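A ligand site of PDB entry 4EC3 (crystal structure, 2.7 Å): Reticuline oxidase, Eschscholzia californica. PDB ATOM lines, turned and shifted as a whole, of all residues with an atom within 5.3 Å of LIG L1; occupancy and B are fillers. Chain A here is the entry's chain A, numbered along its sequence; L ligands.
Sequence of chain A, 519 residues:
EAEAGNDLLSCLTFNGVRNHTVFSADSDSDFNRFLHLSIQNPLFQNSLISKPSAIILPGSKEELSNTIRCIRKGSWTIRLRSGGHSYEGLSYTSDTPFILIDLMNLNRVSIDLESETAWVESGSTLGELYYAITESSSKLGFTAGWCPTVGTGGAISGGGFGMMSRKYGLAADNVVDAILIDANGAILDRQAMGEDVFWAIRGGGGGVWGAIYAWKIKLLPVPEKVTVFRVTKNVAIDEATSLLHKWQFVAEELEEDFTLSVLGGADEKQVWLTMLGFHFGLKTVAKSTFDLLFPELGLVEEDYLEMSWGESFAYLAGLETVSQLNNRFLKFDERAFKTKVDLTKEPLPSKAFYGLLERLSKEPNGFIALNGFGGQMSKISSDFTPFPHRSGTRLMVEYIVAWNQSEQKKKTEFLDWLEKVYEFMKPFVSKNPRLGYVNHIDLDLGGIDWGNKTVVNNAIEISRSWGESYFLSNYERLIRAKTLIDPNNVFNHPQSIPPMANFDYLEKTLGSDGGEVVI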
ATOM      1  N   TYR A  87     -21.841  23.352   1.823  1.00  0.00           N
ATOM      2  CA  TYR A  87     -21.202  22.195   1.217  1.00  0.00           C
ATOM      3  C   TYR A  87     -20.457  21.363   2.243  1.00  0.00           C
ATOM      4  O   TYR A  87     -20.171  20.191   2.015  1.00  0.00           O
ATOM      5  CB  TYR A  87     -20.246  22.632   0.108  1.00  0.00           C
ATOM      6  CG  TYR A  87     -20.940  23.272  -1.069  1.00  0.00           C
ATOM      7  CD1 TYR A  87     -22.284  23.045  -1.316  1.00  0.00           C
ATOM      8  CD2 TYR A  87     -20.243  24.115  -1.929  1.00  0.00           C
ATOM      9  CE1 TYR A  87     -22.925  23.630  -2.390  1.00  0.00           C
ATOM     10  CE2 TYR A  87     -20.877  24.707  -3.013  1.00  0.00           C
ATOM     11  CZ  TYR A  87     -22.212  24.465  -3.234  1.00  0.00           C
ATOM     12  OH  TYR A  87     -22.842  25.052  -4.299  1.00  0.00           O
ATOM     13  N   TRP A 146     -28.970  29.198  -8.980  1.00  0.00           N
ATOM     14  CA  TRP A 146     -29.844  28.318  -9.740  1.00  0.00           C
ATOM     15  C   TRP A 146     -30.550  27.252  -8.893  1.00  0.00           C
ATOM     16  O   TRP A 146     -31.285  26.423  -9.423  1.00  0.00           O
ATOM     17  CB  TRP A 146     -29.068  27.626 -10.866  1.00  0.00           C
ATOM     18  CG  TRP A 146     -28.263  28.543 -11.746  1.00  0.00           C
ATOM     19  CD1 TRP A 146     -27.134  29.231 -11.420  1.00  0.00           C
ATOM     20  CD2 TRP A 146     -28.531  28.848 -13.129  1.00  0.00           C
ATOM     21  NE1 TRP A 146     -26.687  29.958 -12.488  1.00  0.00           N
ATOM     22  CE2 TRP A 146     -27.520  29.740 -13.557  1.00  0.00           C
ATOM     23  CE3 TRP A 146     -29.520  28.462 -14.038  1.00  0.00           C
ATOM     24  CZ2 TRP A 146     -27.473  30.248 -14.856  1.00  0.00           C
ATOM     25  CZ3 TRP A 146     -29.472  28.967 -15.327  1.00  0.00           C
ATOM     26  CH2 TRP A 146     -28.454  29.850 -15.717  1.00  0.00           C
ATOM     27  N   CYS A 147     -30.313  27.263  -7.592  1.00  0.00           N
ATOM     28  CA  CYS A 147     -30.927  26.261  -6.724  1.00  0.00           C
ATOM     29  C   CYS A 147     -32.016  26.870  -5.829  1.00  0.00           C
ATOM     30  O   CYS A 147     -31.724  27.683  -4.949  1.00  0.00           O
ATOM     31  CB  CYS A 147     -29.860  25.558  -5.874  1.00  0.00           C
ATOM     32  SG  CYS A 147     -28.499  24.771  -6.805  1.00  0.00           S
ATOM     33  N   SER A 261     -24.957  28.856 -19.627  1.00  0.00           N
ATOM     34  CA  SER A 261     -24.233  28.017 -18.683  1.00  0.00           C
ATOM     35  C   SER A 261     -24.278  26.559 -19.118  1.00  0.00           C
ATOM     36  O   SER A 261     -25.179  26.165 -19.866  1.00  0.00           O
ATOM     37  CB  SER A 261     -24.790  28.172 -17.269  1.00  0.00           C
ATOM     38  OG  SER A 261     -24.362  29.403 -16.692  1.00  0.00           O
ATOM     39  N   VAL A 262     -23.333  25.766 -18.637  1.00  0.00           N
ATOM     40  CA  VAL A 262     -23.220  24.373 -19.061  1.00  0.00           C
ATOM     41  C   VAL A 262     -23.132  23.403 -17.890  1.00  0.00           C
ATOM     42  O   VAL A 262     -22.307  23.560 -17.002  1.00  0.00           O
ATOM     43  CB  VAL A 262     -21.989  24.161 -19.982  1.00  0.00           C
ATOM     44  CG1 VAL A 262     -21.822  22.692 -20.309  1.00  0.00           C
ATOM     45  CG2 VAL A 262     -22.120  24.969 -21.260  1.00  0.00           C
ATOM     46  N   LEU A 263     -23.984  22.396 -17.892  1.00  0.00           N
ATOM     47  CA  LEU A 263     -23.750  21.235 -17.045  1.00  0.00           C
ATOM     48  C   LEU A 263     -23.126  20.177 -17.936  1.00  0.00           C
ATOM     49  O   LEU A 263     -23.451  20.103 -19.114  1.00  0.00           O
ATOM     50  CB  LEU A 263     -25.052  20.739 -16.427  1.00  0.00           C
ATOM     51  CG  LEU A 263     -25.614  21.689 -15.364  1.00  0.00           C
ATOM     52  CD1 LEU A 263     -26.979  21.242 -14.880  1.00  0.00           C
ATOM     53  CD2 LEU A 263     -24.630  21.792 -14.213  1.00  0.00           C
ATOM     54  N   LEU A 276     -27.816  25.333 -20.725  1.00  0.00           N
ATOM     55  CA  LEU A 276     -28.835  26.159 -20.090  1.00  0.00           C
ATOM     56  C   LEU A 276     -28.684  27.575 -20.590  1.00  0.00           C
ATOM     57  O   LEU A 276     -27.722  28.263 -20.238  1.00  0.00           O
ATOM     58  CB  LEU A 276     -28.680  26.124 -18.567  1.00  0.00           C
ATOM     59  CG  LEU A 276     -28.610  24.746 -17.915  1.00  0.00           C
ATOM     60  CD1 LEU A 276     -28.304  24.874 -16.439  1.00  0.00           C
ATOM     61  CD2 LEU A 276     -29.900  23.985 -18.129  1.00  0.00           C
ATOM     62  N   PHE A 332     -33.445  18.751  -4.261  1.00  0.00           N
ATOM     63  CA  PHE A 332     -32.856  18.930  -5.575  1.00  0.00           C
ATOM     64  C   PHE A 332     -32.123  17.667  -6.003  1.00  0.00           C
ATOM     65  O   PHE A 332     -32.100  17.314  -7.183  1.00  0.00           O
ATOM     66  CB  PHE A 332     -31.866  20.106  -5.552  1.00  0.00           C
ATOM     67  CG  PHE A 332     -30.660  19.854  -4.684  1.00  0.00           C
ATOM     68  CD1 PHE A 332     -30.733  20.010  -3.306  1.00  0.00           C
ATOM     69  CD2 PHE A 332     -29.459  19.461  -5.249  1.00  0.00           C
ATOM     70  CE1 PHE A 332     -29.626  19.769  -2.513  1.00  0.00           C
ATOM     71  CE2 PHE A 332     -28.338  19.216  -4.459  1.00  0.00           C
ATOM     72  CZ  PHE A 332     -28.426  19.378  -3.088  1.00  0.00           C
ATOM     73  N   ASP A 333     -31.531  16.974  -5.032  1.00  0.00           N
ATOM     74  CA  ASP A 333     -30.731  15.788  -5.275  1.00  0.00           C
ATOM     75  C   ASP A 333     -30.504  15.060  -3.950  1.00  0.00           C
ATOM     76  O   ASP A 333     -29.985  15.635  -2.991  1.00  0.00           O
ATOM     77  CB  ASP A 333     -29.398  16.156  -5.919  1.00  0.00           C
ATOM     78  CG  ASP A 333     -28.779  15.028  -6.713  1.00  0.00           C
ATOM     79  OD1 ASP A 333     -28.156  15.309  -7.756  1.00  0.00           O
ATOM     80  OD2 ASP A 333     -28.913  13.856  -6.289  1.00  0.00           O
ATOM     81  N   ARG A 335     -28.481  12.835  -3.223  1.00  0.00           N
ATOM     82  CA  ARG A 335     -27.134  12.289  -3.110  1.00  0.00           C
ATOM     83  C   ARG A 335     -26.191  13.147  -2.283  1.00  0.00           C
ATOM     84  O   ARG A 335     -26.176  14.370  -2.414  1.00  0.00           O
ATOM     85  CB  ARG A 335     -26.531  12.066  -4.497  1.00  0.00           C
ATOM     86  CG  ARG A 335     -27.229  11.017  -5.328  1.00  0.00           C
ATOM     87  CD  ARG A 335     -26.619  10.976  -6.722  1.00  0.00           C
ATOM     88  NE  ARG A 335     -26.715  12.273  -7.380  1.00  0.00           N
ATOM     89  CZ  ARG A 335     -26.044  12.609  -8.479  1.00  0.00           C
ATOM     90  NH1 ARG A 335     -25.219  11.746  -9.051  1.00  0.00           N
ATOM     91  NH2 ARG A 335     -26.203  13.818  -9.004  1.00  0.00           N
ATOM     92  N   ALA A 336     -25.398  12.494  -1.439  1.00  0.00           N
ATOM     93  CA  ALA A 336     -24.294  13.142  -0.754  1.00  0.00           C
ATOM     94  C   ALA A 336     -23.292  13.584  -1.807  1.00  0.00           C
ATOM     95  O   ALA A 336     -23.055  12.874  -2.788  1.00  0.00           O
ATOM     96  CB  ALA A 336     -23.643  12.185   0.224  1.00  0.00           C
ATOM     97  N   PHE A 337     -22.707  14.769  -1.622  1.00  0.00           N
ATOM     98  CA  PHE A 337     -21.807  15.298  -2.636  1.00  0.00           C
ATOM     99  C   PHE A 337     -20.596  16.016  -2.066  1.00  0.00           C
ATOM    100  O   PHE A 337     -20.566  16.397  -0.888  1.00  0.00           O
ATOM    101  CB  PHE A 337     -22.565  16.248  -3.578  1.00  0.00           C
ATOM    102  CG  PHE A 337     -23.062  17.503  -2.908  1.00  0.00           C
ATOM    103  CD1 PHE A 337     -22.302  18.664  -2.946  1.00  0.00           C
ATOM    104  CD2 PHE A 337     -24.278  17.518  -2.248  1.00  0.00           C
ATOM    105  CE1 PHE A 337     -22.758  19.818  -2.329  1.00  0.00           C
ATOM    106  CE2 PHE A 337     -24.740  18.682  -1.638  1.00  0.00           C
ATOM    107  CZ  PHE A 337     -23.970  19.823  -1.671  1.00  0.00           C
ATOM    108  N   THR A 339     -17.998  19.144  -3.710  1.00  0.00           N
ATOM    109  CA  THR A 339     -17.786  20.014  -4.860  1.00  0.00           C
ATOM    110  C   THR A 339     -16.701  21.043  -4.608  1.00  0.00           C
ATOM    111  O   THR A 339     -16.646  21.673  -3.538  1.00  0.00           O
ATOM    112  CB  THR A 339     -19.099  20.717  -5.284  1.00  0.00           C
ATOM    113  OG1 THR A 339     -18.834  21.642  -6.345  1.00  0.00           O
ATOM    114  CG2 THR A 339     -19.730  21.457  -4.117  1.00  0.00           C
ATOM    115  N   PHE A 367     -19.582  15.307 -12.331  1.00  0.00           N
ATOM    116  CA  PHE A 367     -20.049  16.234 -13.357  1.00  0.00           C
ATOM    117  C   PHE A 367     -19.483  17.633 -13.104  1.00  0.00           C
ATOM    118  O   PHE A 367     -18.988  17.917 -12.016  1.00  0.00           O
ATOM    119  CB  PHE A 367     -21.575  16.235 -13.475  1.00  0.00           C
ATOM    120  CG  PHE A 367     -22.300  16.748 -12.266  1.00  0.00           C
ATOM    121  CD1 PHE A 367     -22.772  18.049 -12.215  1.00  0.00           C
ATOM    122  CD2 PHE A 367     -22.556  15.914 -11.183  1.00  0.00           C
ATOM    123  CE1 PHE A 367     -23.453  18.514 -11.110  1.00  0.00           C
ATOM    124  CE2 PHE A 367     -23.242  16.388 -10.075  1.00  0.00           C
ATOM    125  CZ  PHE A 367     -23.688  17.683 -10.040  1.00  0.00           C
ATOM    126  N   ALA A 369     -19.945  22.086 -13.812  1.00  0.00           N
ATOM    127  CA  ALA A 369     -20.821  23.210 -14.126  1.00  0.00           C
ATOM    128  C   ALA A 369     -19.955  24.408 -14.496  1.00  0.00           C
ATOM    129  O   ALA A 369     -19.015  24.767 -13.794  1.00  0.00           O
ATOM    130  CB  ALA A 369     -21.728  23.527 -12.959  1.00  0.00           C
ATOM    131  N   ASN A 371     -20.012  28.399 -15.688  1.00  0.00           N
ATOM    132  CA  ASN A 371     -20.728  29.663 -15.795  1.00  0.00           C
ATOM    133  C   ASN A 371     -19.836  30.780 -16.304  1.00  0.00           C
ATOM    134  O   ASN A 371     -18.661  30.861 -15.951  1.00  0.00           O
ATOM    135  CB  ASN A 371     -21.338  30.048 -14.450  1.00  0.00           C
ATOM    136  CG  ASN A 371     -22.544  29.222 -14.098  1.00  0.00           C
ATOM    137  OD1 ASN A 371     -23.655  29.514 -14.523  1.00  0.00           O
ATOM    138  ND2 ASN A 371     -22.332  28.165 -13.314  1.00  0.00           N
ATOM    139  N   MET A 396     -16.594  30.686 -13.971  1.00  0.00           N
ATOM    140  CA  MET A 396     -16.653  29.895 -12.752  1.00  0.00           C
ATOM    141  C   MET A 396     -16.822  28.438 -13.167  1.00  0.00           C
ATOM    142  O   MET A 396     -17.809  28.066 -13.801  1.00  0.00           O
ATOM    143  CB  MET A 396     -17.808  30.327 -11.849  1.00  0.00           C
ATOM    144  CG  MET A 396     -17.829  29.599 -10.516  1.00  0.00           C
ATOM    145  SD  MET A 396     -18.876  30.385  -9.281  1.00  0.00           S
ATOM    146  CE  MET A 396     -20.493  30.199 -10.027  1.00  0.00           C
ATOM    147  N   GLU A 398     -17.034  24.810 -11.651  1.00  0.00           N
ATOM    148  CA  GLU A 398     -17.144  23.940 -10.485  1.00  0.00           C
ATOM    149  C   GLU A 398     -17.222  22.464 -10.847  1.00  0.00           C
ATOM    150  O   GLU A 398     -17.868  22.066 -11.825  1.00  0.00           O
ATOM    151  CB  GLU A 398     -18.313  24.355  -9.585  1.00  0.00           C
ATOM    152  CG  GLU A 398     -19.682  24.220 -10.212  1.00  0.00           C
ATOM    153  CD  GLU A 398     -20.789  24.650  -9.265  1.00  0.00           C
ATOM    154  OE1 GLU A 398     -21.454  25.674  -9.556  1.00  0.00           O
ATOM    155  OE2 GLU A 398     -20.996  23.957  -8.248  1.00  0.00           O
ATOM    156  N   ILE A 400     -18.171  18.732  -9.404  1.00  0.00           N
ATOM    157  CA  ILE A 400     -18.997  18.080  -8.402  1.00  0.00           C
ATOM    158  C   ILE A 400     -18.870  16.569  -8.523  1.00  0.00           C
ATOM    159  O   ILE A 400     -18.822  16.042  -9.636  1.00  0.00           O
ATOM    160  CB  ILE A 400     -20.487  18.444  -8.569  1.00  0.00           C
ATOM    161  CG1 ILE A 400     -20.679  19.954  -8.719  1.00  0.00           C
ATOM    162  CG2 ILE A 400     -21.320  17.901  -7.413  1.00  0.00           C
ATOM    163  CD1 ILE A 400     -20.731  20.426 -10.168  1.00  0.00           C
ATOM    164  N   ALA A 402     -21.029  13.272  -6.827  1.00  0.00           N
ATOM    165  CA  ALA A 402     -22.149  12.897  -5.978  1.00  0.00           C
ATOM    166  C   ALA A 402     -22.384  11.393  -6.008  1.00  0.00           C
ATOM    167  O   ALA A 402     -21.943  10.707  -6.922  1.00  0.00           O
ATOM    168  CB  ALA A 402     -23.413  13.632  -6.422  1.00  0.00           C
ATOM    169  N   HIS A 440     -19.164  28.719  -1.971  1.00  0.00           N
ATOM    170  CA  HIS A 440     -18.652  27.428  -2.371  1.00  0.00           C
ATOM    171  C   HIS A 440     -17.573  27.014  -1.387  1.00  0.00           C
ATOM    172  O   HIS A 440     -16.478  26.618  -1.790  1.00  0.00           O
ATOM    173  CB  HIS A 440     -18.081  27.504  -3.791  1.00  0.00           C
ATOM    174  CG  HIS A 440     -18.212  26.235  -4.571  1.00  0.00           C
ATOM    175  ND1 HIS A 440     -17.391  25.144  -4.365  1.00  0.00           N
ATOM    176  CD2 HIS A 440     -19.053  25.885  -5.568  1.00  0.00           C
ATOM    177  CE1 HIS A 440     -17.726  24.177  -5.203  1.00  0.00           C
ATOM    178  NE2 HIS A 440     -18.735  24.600  -5.935  1.00  0.00           N
HETATM  179  C1  LIG L   1     -26.262  19.934  -8.436  1.00  0.00           C
HETATM  180  C2  LIG L   1     -26.410  18.594  -8.020  1.00  0.00           C
HETATM  181  C3  LIG L   1     -25.704  18.122  -6.939  1.00  0.00           C
HETATM  182  C4  LIG L   1     -24.838  18.949  -6.243  1.00  0.00           C
HETATM  183  C5  LIG L   1     -24.681  20.273  -6.632  1.00  0.00           C
HETATM  184  C6  LIG L   1     -23.734  21.164  -5.860  1.00  0.00           C
HETATM  185  C7  LIG L   1     -23.138  22.085  -6.862  1.00  0.00           C
HETATM  186  N1  LIG L   1     -24.243  22.862  -7.331  1.00  0.00           N
HETATM  187  C8  LIG L   1     -25.248  22.207  -8.191  1.00  0.00           C
HETATM  188  C9  LIG L   1     -24.891  22.169  -9.700  1.00  0.00           C
HETATM  189  C10 LIG L   1     -25.202  23.410 -10.588  1.00  0.00           C
HETATM  190  C11 LIG L   1     -26.307  23.426 -11.438  1.00  0.00           C
HETATM  191  C12 LIG L   1     -26.561  24.543 -12.221  1.00  0.00           C
HETATM  192  C13 LIG L   1     -25.696  25.660 -12.141  1.00  0.00           C
HETATM  193  O1  LIG L   1     -25.924  26.771 -12.898  1.00  0.00           O
HETATM  194  C14 LIG L   1     -26.017  26.652 -14.291  1.00  0.00           C
HETATM  195  C15 LIG L   1     -24.621  25.635 -11.308  1.00  0.00           C
HETATM  196  O2  LIG L   1     -23.779  26.731 -11.240  1.00  0.00           O
HETATM  197  C16 LIG L   1     -24.362  24.509 -10.529  1.00  0.00           C
HETATM  198  C17 LIG L   1     -25.411  20.767  -7.746  1.00  0.00           C
HETATM  199  C18 LIG L   1     -24.048  24.297  -7.156  1.00  0.00           C
HETATM  200  O3  LIG L   1     -25.859  16.796  -6.540  1.00  0.00           O
HETATM  201  C19 LIG L   1     -25.845  16.458  -5.165  1.00  0.00           C
HETATM  202  O4  LIG L   1     -27.264  17.745  -8.703  1.00  0.00           O
HETATM  203  P1  LG2 L   2     -26.825  27.268   5.242  1.00  0.00           P
HETATM  204  O1  LG2 L   2     -25.976  26.063   5.551  1.00  0.00           O
HETATM  205  O2  LG2 L   2     -28.015  27.378   6.183  1.00  0.00           O
HETATM  206  O3  LG2 L   2     -25.921  28.590   5.295  1.00  0.00           O
HETATM  207  C1  LG2 L   2     -24.564  28.558   4.900  1.00  0.00           C
HETATM  208  C2  LG2 L   2     -23.708  29.375   5.856  1.00  0.00           C
HETATM  209  O4  LG2 L   2     -24.338  30.606   6.155  1.00  0.00           O
HETATM  210  C3  LG2 L   2     -23.518  28.653   7.177  1.00  0.00           C
HETATM  211  O5  LG2 L   2     -22.229  28.934   7.666  1.00  0.00           O
HETATM  212  C4  LG2 L   2     -24.548  29.279   8.077  1.00  0.00           C
HETATM  213  O6  LG2 L   2     -24.124  29.279   9.418  1.00  0.00           O
HETATM  214  C5  LG2 L   2     -24.677  30.687   7.525  1.00  0.00           C
HETATM  215  N1  LG2 L   2     -26.045  31.184   7.706  1.00  0.00           N
HETATM  216  C6  LG2 L   2     -27.209  30.501   7.450  1.00  0.00           C
HETATM  217  N2  LG2 L   2     -28.251  31.310   7.751  1.00  0.00           N
HETATM  218  C7  LG2 L   2     -27.771  32.496   8.193  1.00  0.00           C
HETATM  219  C8  LG2 L   2     -28.397  33.661   8.621  1.00  0.00           C
HETATM  220  N3  LG2 L   2     -29.662  33.865   8.293  1.00  0.00           N
HETATM  221  N4  LG2 L   2     -27.620  34.729   9.027  1.00  0.00           N
HETATM  222  C9  LG2 L   2     -26.247  34.643   8.991  1.00  0.00           C
HETATM  223  N5  LG2 L   2     -25.635  33.484   8.557  1.00  0.00           N
HETATM  224  C10 LG2 L   2     -26.382  32.426   8.169  1.00  0.00           C
HETATM  225  N6  LG2 L   2     -24.429  29.464  -4.845  1.00  0.00           N
HETATM  226  C11 LG2 L   2     -24.418  30.405  -5.850  1.00  0.00           C
HETATM  227  O7  LG2 L   2     -23.870  31.488  -5.665  1.00  0.00           O
HETATM  228  N7  LG2 L   2     -25.043  30.149  -7.046  1.00  0.00           N
HETATM  229  C12 LG2 L   2     -25.671  28.938  -7.252  1.00  0.00           C
HETATM  230  O8  LG2 L   2     -26.215  28.707  -8.329  1.00  0.00           O
HETATM  231  C13 LG2 L   2     -25.685  27.981  -6.239  1.00  0.00           C
HETATM  232  N8  LG2 L   2     -26.328  26.778  -6.419  1.00  0.00           N
HETATM  233  C14 LG2 L   2     -26.473  25.904  -5.364  1.00  0.00           C
HETATM  234  C15 LG2 L   2     -27.270  24.781  -5.530  1.00  0.00           C
HETATM  235  C16 LG2 L   2     -27.370  23.884  -4.477  1.00  0.00           C
HETATM  236  C17 LG2 L   2     -28.142  22.622  -4.714  1.00  0.00           C
HETATM  237  C18 LG2 L   2     -26.805  24.150  -3.227  1.00  0.00           C
HETATM  238  C19 LG2 L   2     -27.031  23.221  -2.058  1.00  0.00           C
HETATM  239  C20 LG2 L   2     -26.037  25.308  -3.069  1.00  0.00           C
HETATM  240  C21 LG2 L   2     -25.838  26.162  -4.158  1.00  0.00           C
HETATM  241  N9  LG2 L   2     -25.091  27.315  -4.018  1.00  0.00           N
HETATM  242  C22 LG2 L   2     -25.094  28.260  -5.021  1.00  0.00           C
HETATM  243  C23 LG2 L   2     -24.277  27.557  -2.773  1.00  0.00           C
HETATM  244  C24 LG2 L   2     -25.007  28.477  -1.806  1.00  0.00           C
HETATM  245  O9  LG2 L   2     -24.943  29.826  -2.236  1.00  0.00           O
HETATM  246  C25 LG2 L   2     -24.347  28.351  -0.430  1.00  0.00           C
HETATM  247  O10 LG2 L   2     -24.328  26.989  -0.079  1.00  0.00           O
HETATM  248  C26 LG2 L   2     -25.111  29.145   0.615  1.00  0.00           C
HETATM  249  O11 LG2 L   2     -24.213  29.580   1.624  1.00  0.00           O
HETATM  250  C27 LG2 L   2     -26.199  28.279   1.230  1.00  0.00           C
HETATM  251  O12 LG2 L   2     -26.995  29.019   2.110  1.00  0.00           O
HETATM  252  P2  LG2 L   2     -28.139  28.252   2.937  1.00  0.00           P
HETATM  253  O13 LG2 L   2     -28.837  29.195   3.884  1.00  0.00           O
HETATM  254  O14 LG2 L   2     -29.130  27.608   1.994  1.00  0.00           O
HETATM  255  O15 LG2 L   2     -27.305  27.126   3.717  1.00  0.00           O
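OH of Tyr 87 touches C18 of LIG L1, 3.2 Å away.
Ser 261 touches LIG L1 (CB to C14, 3.6 Å).
Leu 263 touches LIG L1 (CD2 to C11, 3.6 Å).
CD1 of Leu 276 touches C14 of LIG L1, 3.6 Å away.
CE2 of Phe 332 touches C3 of LIG L1, at 3.8 Å.
Arg 335 touches LIG L1 (O to C19, 3.5 Å).
Phe 337 touches LIG L1.
CZ of Phe 367 touches C2 of LIG L1, at 3.5 Å.
Ala 369 touches LIG L1 (CB to C16, 3.7 Å).
CG1 of Ile 400 touches C7 of LIG L1, at 3.7 Å.
CB of Ala 402 touches C19 of LIG L1, at 3.9 Å.
Hydrophobic or aromatic side chains within 4 Å of LIG L1: Trp 146, Leu 263, Leu 276, Phe 332, Phe 337, Phe 367, Ala 369, Ile 400 and Ala 402.
15 residues have an atom within 4 Å of LIG L1: Tyr 87, Trp 146, Ser 261, Leu 263, Leu 276, Phe 332, Asp 333, Arg 335, Phe 337, Phe 367, Ala 369, Asn 371, Glu 398, Ile 400 and Ala 402.
The side-chain carboxylate (OD1) of Asp 333 is in salt-bridge range of the guanidinium group (NH2) of Arg 335 (2.8 Å).
N of Met 396 lies within hydrogen-bond range of O of Asn 371.
The backbone NH of Ala 369 lies within hydrogen-bond range of the backbone carbonyl oxygen of Glu 398 (2.9 Å).
The side-chain carboxylate (OE2) of Glu 398 is in hydrogen-bond range of a ring nitrogen (NE2) of His 440, at 3.3 Å.
The backbone NH (N) of Ile 400 sits at hydrogen-bond distance from the backbone carbonyl oxygen (O) of Phe 367, 2.9 Å away.
The backbone NH of Ser 261 sits at hydrogen-bond distance from the backbone carbonyl oxygen of Leu 276, 2.9 Å away.
An oxygen (O4) of LIG L1 lies within hydrogen-bond range of the side-chain carboxylate of Asp 333, at 2.8 Å.
An oxygen (O2) of LIG L1 lies within hydrogen-bond range of the side-chain amide nitrogen (ND2) of Asn 371, 2.9 Å away.
OE2 of Glu 398 is in salt-bridge range of N1 of LIG L1 (3.5 Å).
NE1 of Trp 146 sits close to O1 of LIG L1 (3.3 Å).
The backbone NH (N) of Trp 146 sits at hydrogen-bond distance from an oxygen (O8) of LG2 L2, at 2.9 Å.
The side-chain sulfur (SG) of Cys 147 is covalently linked to a carbon (C15) of LG2 L2 (1.8 Å).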
